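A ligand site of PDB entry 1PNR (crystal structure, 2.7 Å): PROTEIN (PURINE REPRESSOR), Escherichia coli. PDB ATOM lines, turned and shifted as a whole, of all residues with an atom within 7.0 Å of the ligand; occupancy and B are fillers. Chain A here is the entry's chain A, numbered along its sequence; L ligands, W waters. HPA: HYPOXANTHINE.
O of Asp 274 lies within hydrogen-bond range of N of Gln 291, at 3.2 Å.
The guanidinium group of Arg 195 sits at hydrogen-bond distance from the backbone carbonyl oxygen of Gly 245.
OD1 of Asp 274 is in salt-bridge range of NH2 of Arg 195, 2.6 Å away.
NH1 of Arg 189 is in salt-bridge range of OE2 of Glu 124, 2.8 Å away.
The side-chain hydroxyl of Tyr 72 is in hydrogen-bond range of the side-chain amide oxygen of Gln 291 (3.0 Å).
A nitrogen (N7) of the ligand lies within hydrogen-bond range of the side-chain hydroxyl (OG1) of Thr 191.
The side-chain carboxylate of Asp 274 lies within hydrogen-bond range of a nitrogen (N9) of the ligand, at 2.9 Å.
The guanidinium group (NE) of Arg 189 lies within hydrogen-bond range of an oxygen (O6) of the ligand, 3.0 Å away.
Water W1 bridges NH2 of Arg 189 (2.6 Å) and N1 of the ligand (3.0 Å).
Merely in contact with the ligand: Tyr 72 (3.1 Å), Phe 73 (3.3 Å), Arg 195 (3.4 Å) and Phe 220 (3.1 Å).
Hydrophobic or aromatic side chains that line the ligand: Tyr 72, Phe 73 and Phe 220.
Along chain A the residues within 4 Å of the ligand span positions 72 to 274.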
ATOM      1  N   THR A  66      14.892 -20.197  -9.936  1.00  0.00           N
ATOM      2  CA  THR A  66      14.585 -20.353  -8.507  1.00  0.00           C
ATOM      3  C   THR A  66      14.753 -19.043  -7.744  1.00  0.00           C
ATOM      4  O   THR A  66      13.808 -18.541  -7.095  1.00  0.00           O
ATOM      5  CB  THR A  66      15.415 -21.427  -7.904  1.00  0.00           C
ATOM      6  OG1 THR A  66      15.024 -22.677  -8.493  1.00  0.00           O
ATOM      7  CG2 THR A  66      15.100 -21.485  -6.460  1.00  0.00           C
ATOM      8  N   SER A  67      15.955 -18.473  -7.896  1.00  0.00           N
ATOM      9  CA  SER A  67      16.280 -17.180  -7.305  1.00  0.00           C
ATOM     10  C   SER A  67      17.488 -16.666  -8.084  1.00  0.00           C
ATOM     11  O   SER A  67      18.046 -17.376  -8.893  1.00  0.00           O
ATOM     12  CB  SER A  67      16.483 -17.247  -5.761  1.00  0.00           C
ATOM     13  OG  SER A  67      17.799 -17.582  -5.324  1.00  0.00           O
ATOM     14  N   ALA A  70      21.865 -15.876  -5.141  1.00  0.00           N
ATOM     15  CA  ALA A  70      22.872 -16.918  -4.960  1.00  0.00           C
ATOM     16  C   ALA A  70      23.930 -17.019  -6.076  1.00  0.00           C
ATOM     17  O   ALA A  70      23.609 -17.253  -7.283  1.00  0.00           O
ATOM     18  CB  ALA A  70      22.160 -18.258  -4.843  1.00  0.00           C
ATOM     19  N   ALA A  71      25.152 -16.833  -5.605  1.00  0.00           N
ATOM     20  CA  ALA A  71      26.342 -16.846  -6.422  1.00  0.00           C
ATOM     21  C   ALA A  71      26.226 -17.831  -7.535  1.00  0.00           C
ATOM     22  O   ALA A  71      26.294 -17.423  -8.677  1.00  0.00           O
ATOM     23  CB  ALA A  71      27.600 -17.147  -5.524  1.00  0.00           C
ATOM     24  N   TYR A  72      26.016 -19.092  -7.156  1.00  0.00           N
ATOM     25  CA  TYR A  72      25.902 -20.190  -8.083  1.00  0.00           C
ATOM     26  C   TYR A  72      24.947 -19.725  -9.216  1.00  0.00           C
ATOM     27  O   TYR A  72      25.330 -19.396 -10.344  1.00  0.00           O
ATOM     28  CB  TYR A  72      25.414 -21.406  -7.309  1.00  0.00           C
ATOM     29  CG  TYR A  72      25.220 -22.628  -8.141  1.00  0.00           C
ATOM     30  CD1 TYR A  72      26.267 -23.249  -8.803  1.00  0.00           C
ATOM     31  CD2 TYR A  72      23.993 -23.149  -8.308  1.00  0.00           C
ATOM     32  CE1 TYR A  72      26.042 -24.414  -9.635  1.00  0.00           C
ATOM     33  CE2 TYR A  72      23.799 -24.257  -9.103  1.00  0.00           C
ATOM     34  CZ  TYR A  72      24.794 -24.885  -9.771  1.00  0.00           C
ATOM     35  OH  TYR A  72      24.446 -25.967 -10.494  1.00  0.00           O
ATOM     36  N   PHE A  73      23.696 -19.628  -8.875  1.00  0.00           N
ATOM     37  CA  PHE A  73      22.717 -19.184  -9.818  1.00  0.00           C
ATOM     38  C   PHE A  73      23.055 -17.954 -10.571  1.00  0.00           C
ATOM     39  O   PHE A  73      22.869 -17.797 -11.771  1.00  0.00           O
ATOM     40  CB  PHE A  73      21.551 -18.727  -8.975  1.00  0.00           C
ATOM     41  CG  PHE A  73      20.852 -19.887  -8.393  1.00  0.00           C
ATOM     42  CD1 PHE A  73      20.975 -21.110  -9.012  1.00  0.00           C
ATOM     43  CD2 PHE A  73      20.145 -19.801  -7.229  1.00  0.00           C
ATOM     44  CE1 PHE A  73      20.365 -22.227  -8.522  1.00  0.00           C
ATOM     45  CE2 PHE A  73      19.504 -20.924  -6.681  1.00  0.00           C
ATOM     46  CZ  PHE A  73      19.660 -22.144  -7.275  1.00  0.00           C
ATOM     47  N   SER A 123      15.317 -26.257  -9.351  1.00  0.00           N
ATOM     48  CA  SER A 123      15.821 -26.874  -8.148  1.00  0.00           C
ATOM     49  C   SER A 123      15.016 -28.025  -7.772  1.00  0.00           C
ATOM     50  O   SER A 123      15.476 -29.095  -7.952  1.00  0.00           O
ATOM     51  CB  SER A 123      15.896 -25.820  -7.022  1.00  0.00           C
ATOM     52  OG  SER A 123      16.777 -24.795  -7.472  1.00  0.00           O
ATOM     53  N   GLU A 124      13.814 -27.856  -7.266  1.00  0.00           N
ATOM     54  CA  GLU A 124      13.101 -29.093  -6.927  1.00  0.00           C
ATOM     55  C   GLU A 124      11.962 -29.369  -7.865  1.00  0.00           C
ATOM     56  O   GLU A 124      11.229 -28.453  -8.213  1.00  0.00           O
ATOM     57  CB  GLU A 124      12.653 -29.043  -5.485  1.00  0.00           C
ATOM     58  CG  GLU A 124      13.870 -28.937  -4.660  1.00  0.00           C
ATOM     59  CD  GLU A 124      13.618 -28.364  -3.314  1.00  0.00           C
ATOM     60  OE1 GLU A 124      12.530 -28.577  -2.746  1.00  0.00           O
ATOM     61  OE2 GLU A 124      14.598 -27.817  -2.786  1.00  0.00           O
ATOM     62  N   ASP A 159      24.867 -32.367 -15.103  1.00  0.00           N
ATOM     63  CA  ASP A 159      26.152 -32.057 -14.442  1.00  0.00           C
ATOM     64  C   ASP A 159      27.029 -33.123 -13.870  1.00  0.00           C
ATOM     65  O   ASP A 159      28.109 -32.782 -13.483  1.00  0.00           O
ATOM     66  CB  ASP A 159      25.970 -30.969 -13.383  1.00  0.00           C
ATOM     67  CG  ASP A 159      25.041 -31.411 -12.268  1.00  0.00           C
ATOM     68  OD1 ASP A 159      24.754 -32.649 -12.290  1.00  0.00           O
ATOM     69  OD2 ASP A 159      24.505 -30.559 -11.506  1.00  0.00           O
ATOM     70  N   PRO A 186      20.137 -29.576   0.179  1.00  0.00           N
ATOM     71  CA  PRO A 186      18.790 -30.208   0.077  1.00  0.00           C
ATOM     72  C   PRO A 186      18.668 -31.487  -0.724  1.00  0.00           C
ATOM     73  O   PRO A 186      19.075 -31.562  -1.890  1.00  0.00           O
ATOM     74  CB  PRO A 186      17.925 -29.126  -0.531  1.00  0.00           C
ATOM     75  CG  PRO A 186      18.671 -27.853  -0.386  1.00  0.00           C
ATOM     76  CD  PRO A 186      20.106 -28.123  -0.036  1.00  0.00           C
ATOM     77  N   ARG A 189      17.054 -31.771  -4.314  1.00  0.00           N
ATOM     78  CA  ARG A 189      17.793 -31.145  -5.389  1.00  0.00           C
ATOM     79  C   ARG A 189      18.903 -32.109  -5.845  1.00  0.00           C
ATOM     80  O   ARG A 189      19.451 -32.890  -5.045  1.00  0.00           O
ATOM     81  CB  ARG A 189      18.525 -29.971  -4.768  1.00  0.00           C
ATOM     82  CG  ARG A 189      17.961 -28.662  -5.241  1.00  0.00           C
ATOM     83  CD  ARG A 189      17.450 -27.826  -4.111  1.00  0.00           C
ATOM     84  NE  ARG A 189      17.963 -26.484  -4.189  1.00  0.00           N
ATOM     85  CZ  ARG A 189      17.349 -25.433  -3.706  1.00  0.00           C
ATOM     86  NH1 ARG A 189      16.164 -25.555  -3.094  1.00  0.00           N
ATOM     87  NH2 ARG A 189      17.830 -24.198  -3.790  1.00  0.00           N
ATOM     88  N   ASN A 190      19.266 -32.065  -7.126  1.00  0.00           N
ATOM     89  CA  ASN A 190      20.324 -32.945  -7.669  1.00  0.00           C
ATOM     90  C   ASN A 190      21.703 -32.628  -7.000  1.00  0.00           C
ATOM     91  O   ASN A 190      22.420 -33.531  -6.519  1.00  0.00           O
ATOM     92  CB  ASN A 190      20.413 -32.709  -9.208  1.00  0.00           C
ATOM     93  CG  ASN A 190      21.518 -33.453  -9.838  1.00  0.00           C
ATOM     94  OD1 ASN A 190      21.701 -34.706  -9.603  1.00  0.00           O
ATOM     95  ND2 ASN A 190      22.317 -32.711 -10.622  1.00  0.00           N
ATOM     96  N   THR A 191      22.040 -31.338  -7.016  1.00  0.00           N
ATOM     97  CA  THR A 191      23.281 -30.808  -6.464  1.00  0.00           C
ATOM     98  C   THR A 191      23.227 -31.088  -4.983  1.00  0.00           C
ATOM     99  O   THR A 191      24.273 -30.918  -4.358  1.00  0.00           O
ATOM    100  CB  THR A 191      23.397 -29.286  -6.525  1.00  0.00           C
ATOM    101  OG1 THR A 191      22.272 -28.689  -5.920  1.00  0.00           O
ATOM    102  CG2 THR A 191      23.575 -28.734  -7.915  1.00  0.00           C
ATOM    103  N   GLY A 192      22.068 -31.506  -4.444  1.00  0.00           N
ATOM    104  CA  GLY A 192      21.985 -31.812  -3.011  1.00  0.00           C
ATOM    105  C   GLY A 192      22.287 -33.313  -2.958  1.00  0.00           C
ATOM    106  O   GLY A 192      23.390 -33.739  -2.770  1.00  0.00           O
ATOM    107  N   ARG A 195      25.300 -35.016  -5.025  1.00  0.00           N
ATOM    108  CA  ARG A 195      26.701 -34.780  -4.706  1.00  0.00           C
ATOM    109  C   ARG A 195      27.044 -35.695  -3.507  1.00  0.00           C
ATOM    110  O   ARG A 195      28.080 -36.314  -3.436  1.00  0.00           O
ATOM    111  CB  ARG A 195      27.001 -33.292  -4.474  1.00  0.00           C
ATOM    112  CG  ARG A 195      26.772 -32.337  -5.648  1.00  0.00           C
ATOM    113  CD  ARG A 195      27.155 -30.795  -5.430  1.00  0.00           C
ATOM    114  NE  ARG A 195      27.011 -29.978  -6.660  1.00  0.00           N
ATOM    115  CZ  ARG A 195      27.003 -28.639  -6.625  1.00  0.00           C
ATOM    116  NH1 ARG A 195      27.127 -28.035  -5.458  1.00  0.00           N
ATOM    117  NH2 ARG A 195      26.854 -27.898  -7.711  1.00  0.00           N
ATOM    118  N   ASP A 219      21.173 -25.763   3.281  1.00  0.00           N
ATOM    119  CA  ASP A 219      20.203 -25.321   2.315  1.00  0.00           C
ATOM    120  C   ASP A 219      20.881 -24.401   1.348  1.00  0.00           C
ATOM    121  O   ASP A 219      20.246 -23.536   0.779  1.00  0.00           O
ATOM    122  CB  ASP A 219      19.162 -24.548   3.115  1.00  0.00           C
ATOM    123  CG  ASP A 219      19.701 -23.280   3.761  1.00  0.00           C
ATOM    124  OD1 ASP A 219      20.800 -22.756   3.488  1.00  0.00           O
ATOM    125  OD2 ASP A 219      18.942 -22.754   4.574  1.00  0.00           O
ATOM    126  N   PHE A 220      22.174 -24.574   1.191  1.00  0.00           N
ATOM    127  CA  PHE A 220      23.015 -23.745   0.315  1.00  0.00           C
ATOM    128  C   PHE A 220      23.324 -22.340   0.789  1.00  0.00           C
ATOM    129  O   PHE A 220      24.164 -21.687   0.217  1.00  0.00           O
ATOM    130  CB  PHE A 220      22.537 -23.699  -1.119  1.00  0.00           C
ATOM    131  CG  PHE A 220      22.683 -25.005  -1.849  1.00  0.00           C
ATOM    132  CD1 PHE A 220      23.907 -25.571  -2.036  1.00  0.00           C
ATOM    133  CD2 PHE A 220      21.549 -25.664  -2.306  1.00  0.00           C
ATOM    134  CE1 PHE A 220      24.036 -26.750  -2.723  1.00  0.00           C
ATOM    135  CE2 PHE A 220      21.666 -26.844  -2.953  1.00  0.00           C
ATOM    136  CZ  PHE A 220      22.943 -27.381  -3.172  1.00  0.00           C
ATOM    137  N   GLU A 221      22.677 -21.878   1.833  1.00  0.00           N
ATOM    138  CA  GLU A 221      22.950 -20.543   2.357  1.00  0.00           C
ATOM    139  C   GLU A 221      23.959 -20.585   3.511  1.00  0.00           C
ATOM    140  O   GLU A 221      23.966 -21.455   4.425  1.00  0.00           O
ATOM    141  CB  GLU A 221      21.634 -19.868   2.797  1.00  0.00           C
ATOM    142  CG  GLU A 221      20.616 -19.498   1.636  1.00  0.00           C
ATOM    143  CD  GLU A 221      20.836 -18.132   0.915  1.00  0.00           C
ATOM    144  OE1 GLU A 221      21.756 -18.025   0.036  1.00  0.00           O
ATOM    145  OE2 GLU A 221      20.024 -17.212   1.197  1.00  0.00           O
ATOM    146  N   GLY A 245      28.798 -29.368   0.738  1.00  0.00           N
ATOM    147  CA  GLY A 245      27.932 -29.381  -0.454  1.00  0.00           C
ATOM    148  C   GLY A 245      27.875 -28.197  -1.410  1.00  0.00           C
ATOM    149  O   GLY A 245      27.526 -28.375  -2.550  1.00  0.00           O
ATOM    150  N   GLY A 246      28.263 -27.021  -0.947  1.00  0.00           N
ATOM    151  CA  GLY A 246      28.296 -25.810  -1.759  1.00  0.00           C
ATOM    152  C   GLY A 246      29.290 -24.772  -1.226  1.00  0.00           C
ATOM    153  O   GLY A 246      29.484 -24.615  -0.037  1.00  0.00           O
ATOM    154  N   ASP A 247      29.930 -24.031  -2.107  1.00  0.00           N
ATOM    155  CA  ASP A 247      30.857 -23.043  -1.647  1.00  0.00           C
ATOM    156  C   ASP A 247      30.331 -21.971  -0.635  1.00  0.00           C
ATOM    157  O   ASP A 247      30.988 -21.583   0.360  1.00  0.00           O
ATOM    158  CB  ASP A 247      31.490 -22.417  -2.857  1.00  0.00           C
ATOM    159  CG  ASP A 247      32.548 -23.265  -3.478  1.00  0.00           C
ATOM    160  OD1 ASP A 247      32.886 -24.335  -2.917  1.00  0.00           O
ATOM    161  OD2 ASP A 247      33.064 -22.874  -4.554  1.00  0.00           O
ATOM    162  N   ILE A 248      29.137 -21.456  -0.900  1.00  0.00           N
ATOM    163  CA  ILE A 248      28.668 -20.448   0.013  1.00  0.00           C
ATOM    164  C   ILE A 248      28.401 -20.943   1.403  1.00  0.00           C
ATOM    165  O   ILE A 248      28.632 -20.287   2.405  1.00  0.00           O
ATOM    166  CB  ILE A 248      27.609 -19.594  -0.595  1.00  0.00           C
ATOM    167  CG1 ILE A 248      28.173 -19.036  -1.894  1.00  0.00           C
ATOM    168  CG2 ILE A 248      26.904 -18.702   0.468  1.00  0.00           C
ATOM    169  CD1 ILE A 248      28.555 -17.573  -2.031  1.00  0.00           C
ATOM    170  N   TYR A 273      32.301 -27.046  -2.915  1.00  0.00           N
ATOM    171  CA  TYR A 273      31.761 -27.461  -4.201  1.00  0.00           C
ATOM    172  C   TYR A 273      31.047 -26.354  -4.882  1.00  0.00           C
ATOM    173  O   TYR A 273      30.142 -25.774  -4.255  1.00  0.00           O
ATOM    174  CB  TYR A 273      30.665 -28.467  -3.975  1.00  0.00           C
ATOM    175  CG  TYR A 273      30.524 -29.323  -5.179  1.00  0.00           C
ATOM    176  CD1 TYR A 273      30.401 -28.791  -6.433  1.00  0.00           C
ATOM    177  CD2 TYR A 273      30.470 -30.721  -5.053  1.00  0.00           C
ATOM    178  CE1 TYR A 273      30.236 -29.637  -7.555  1.00  0.00           C
ATOM    179  CE2 TYR A 273      30.320 -31.538  -6.141  1.00  0.00           C
ATOM    180  CZ  TYR A 273      30.206 -30.995  -7.415  1.00  0.00           C
ATOM    181  OH  TYR A 273      30.025 -31.773  -8.549  1.00  0.00           O
ATOM    182  N   ASP A 274      31.464 -26.134  -6.136  1.00  0.00           N
ATOM    183  CA  ASP A 274      30.908 -25.165  -7.101  1.00  0.00           C
ATOM    184  C   ASP A 274      31.951 -24.348  -7.753  1.00  0.00           C
ATOM    185  O   ASP A 274      31.894 -23.999  -8.927  1.00  0.00           O
ATOM    186  CB  ASP A 274      29.927 -24.202  -6.474  1.00  0.00           C
ATOM    187  CG  ASP A 274      28.516 -24.785  -6.276  1.00  0.00           C
ATOM    188  OD1 ASP A 274      28.261 -25.968  -6.672  1.00  0.00           O
ATOM    189  OD2 ASP A 274      27.692 -24.044  -5.651  1.00  0.00           O
ATOM    190  N   VAL A 276      32.682 -21.243  -6.980  1.00  0.00           N
ATOM    191  CA  VAL A 276      32.110 -19.899  -7.254  1.00  0.00           C
ATOM    192  C   VAL A 276      33.197 -18.887  -7.540  1.00  0.00           C
ATOM    193  O   VAL A 276      34.309 -18.947  -7.014  1.00  0.00           O
ATOM    194  CB  VAL A 276      31.326 -19.388  -6.052  1.00  0.00           C
ATOM    195  CG1 VAL A 276      31.353 -17.863  -5.998  1.00  0.00           C
ATOM    196  CG2 VAL A 276      29.920 -19.856  -6.273  1.00  0.00           C
ATOM    197  N   GLN A 291      32.306 -26.468 -10.927  1.00  0.00           N
ATOM    198  CA  GLN A 291      31.189 -26.702 -11.822  1.00  0.00           C
ATOM    199  C   GLN A 291      31.322 -25.759 -12.957  1.00  0.00           C
ATOM    200  O   GLN A 291      31.398 -24.565 -12.751  1.00  0.00           O
ATOM    201  CB  GLN A 291      29.800 -26.349 -11.306  1.00  0.00           C
ATOM    202  CG  GLN A 291      28.807 -26.846 -12.349  1.00  0.00           C
ATOM    203  CD  GLN A 291      27.883 -27.975 -11.823  1.00  0.00           C
ATOM    204  OE1 GLN A 291      26.786 -27.651 -11.388  1.00  0.00           O
ATOM    205  NE2 GLN A 291      28.348 -29.246 -11.782  1.00  0.00           N
HETATM  206  N1  HPA L   1      21.493 -23.157  -4.712  1.00  0.00           N
HETATM  207  C2  HPA L   1      22.641 -22.412  -4.576  1.00  0.00           C
HETATM  208  N3  HPA L   1      23.844 -22.837  -4.910  1.00  0.00           N
HETATM  209  C4  HPA L   1      23.831 -24.106  -5.392  1.00  0.00           C
HETATM  210  C5  HPA L   1      22.734 -24.922  -5.564  1.00  0.00           C
HETATM  211  C6  HPA L   1      21.450 -24.452  -5.211  1.00  0.00           C
HETATM  212  O6  HPA L   1      20.339 -25.003  -5.272  1.00  0.00           O
HETATM  213  N7  HPA L   1      23.143 -26.139  -6.095  1.00  0.00           N
HETATM  214  C8  HPA L   1      24.447 -26.044  -6.219  1.00  0.00           C
HETATM  215  N9  HPA L   1      24.926 -24.806  -5.833  1.00  0.00           N
HETATM  216  O   HOH W   1      19.295 -22.204  -2.936  1.00  0.00           O
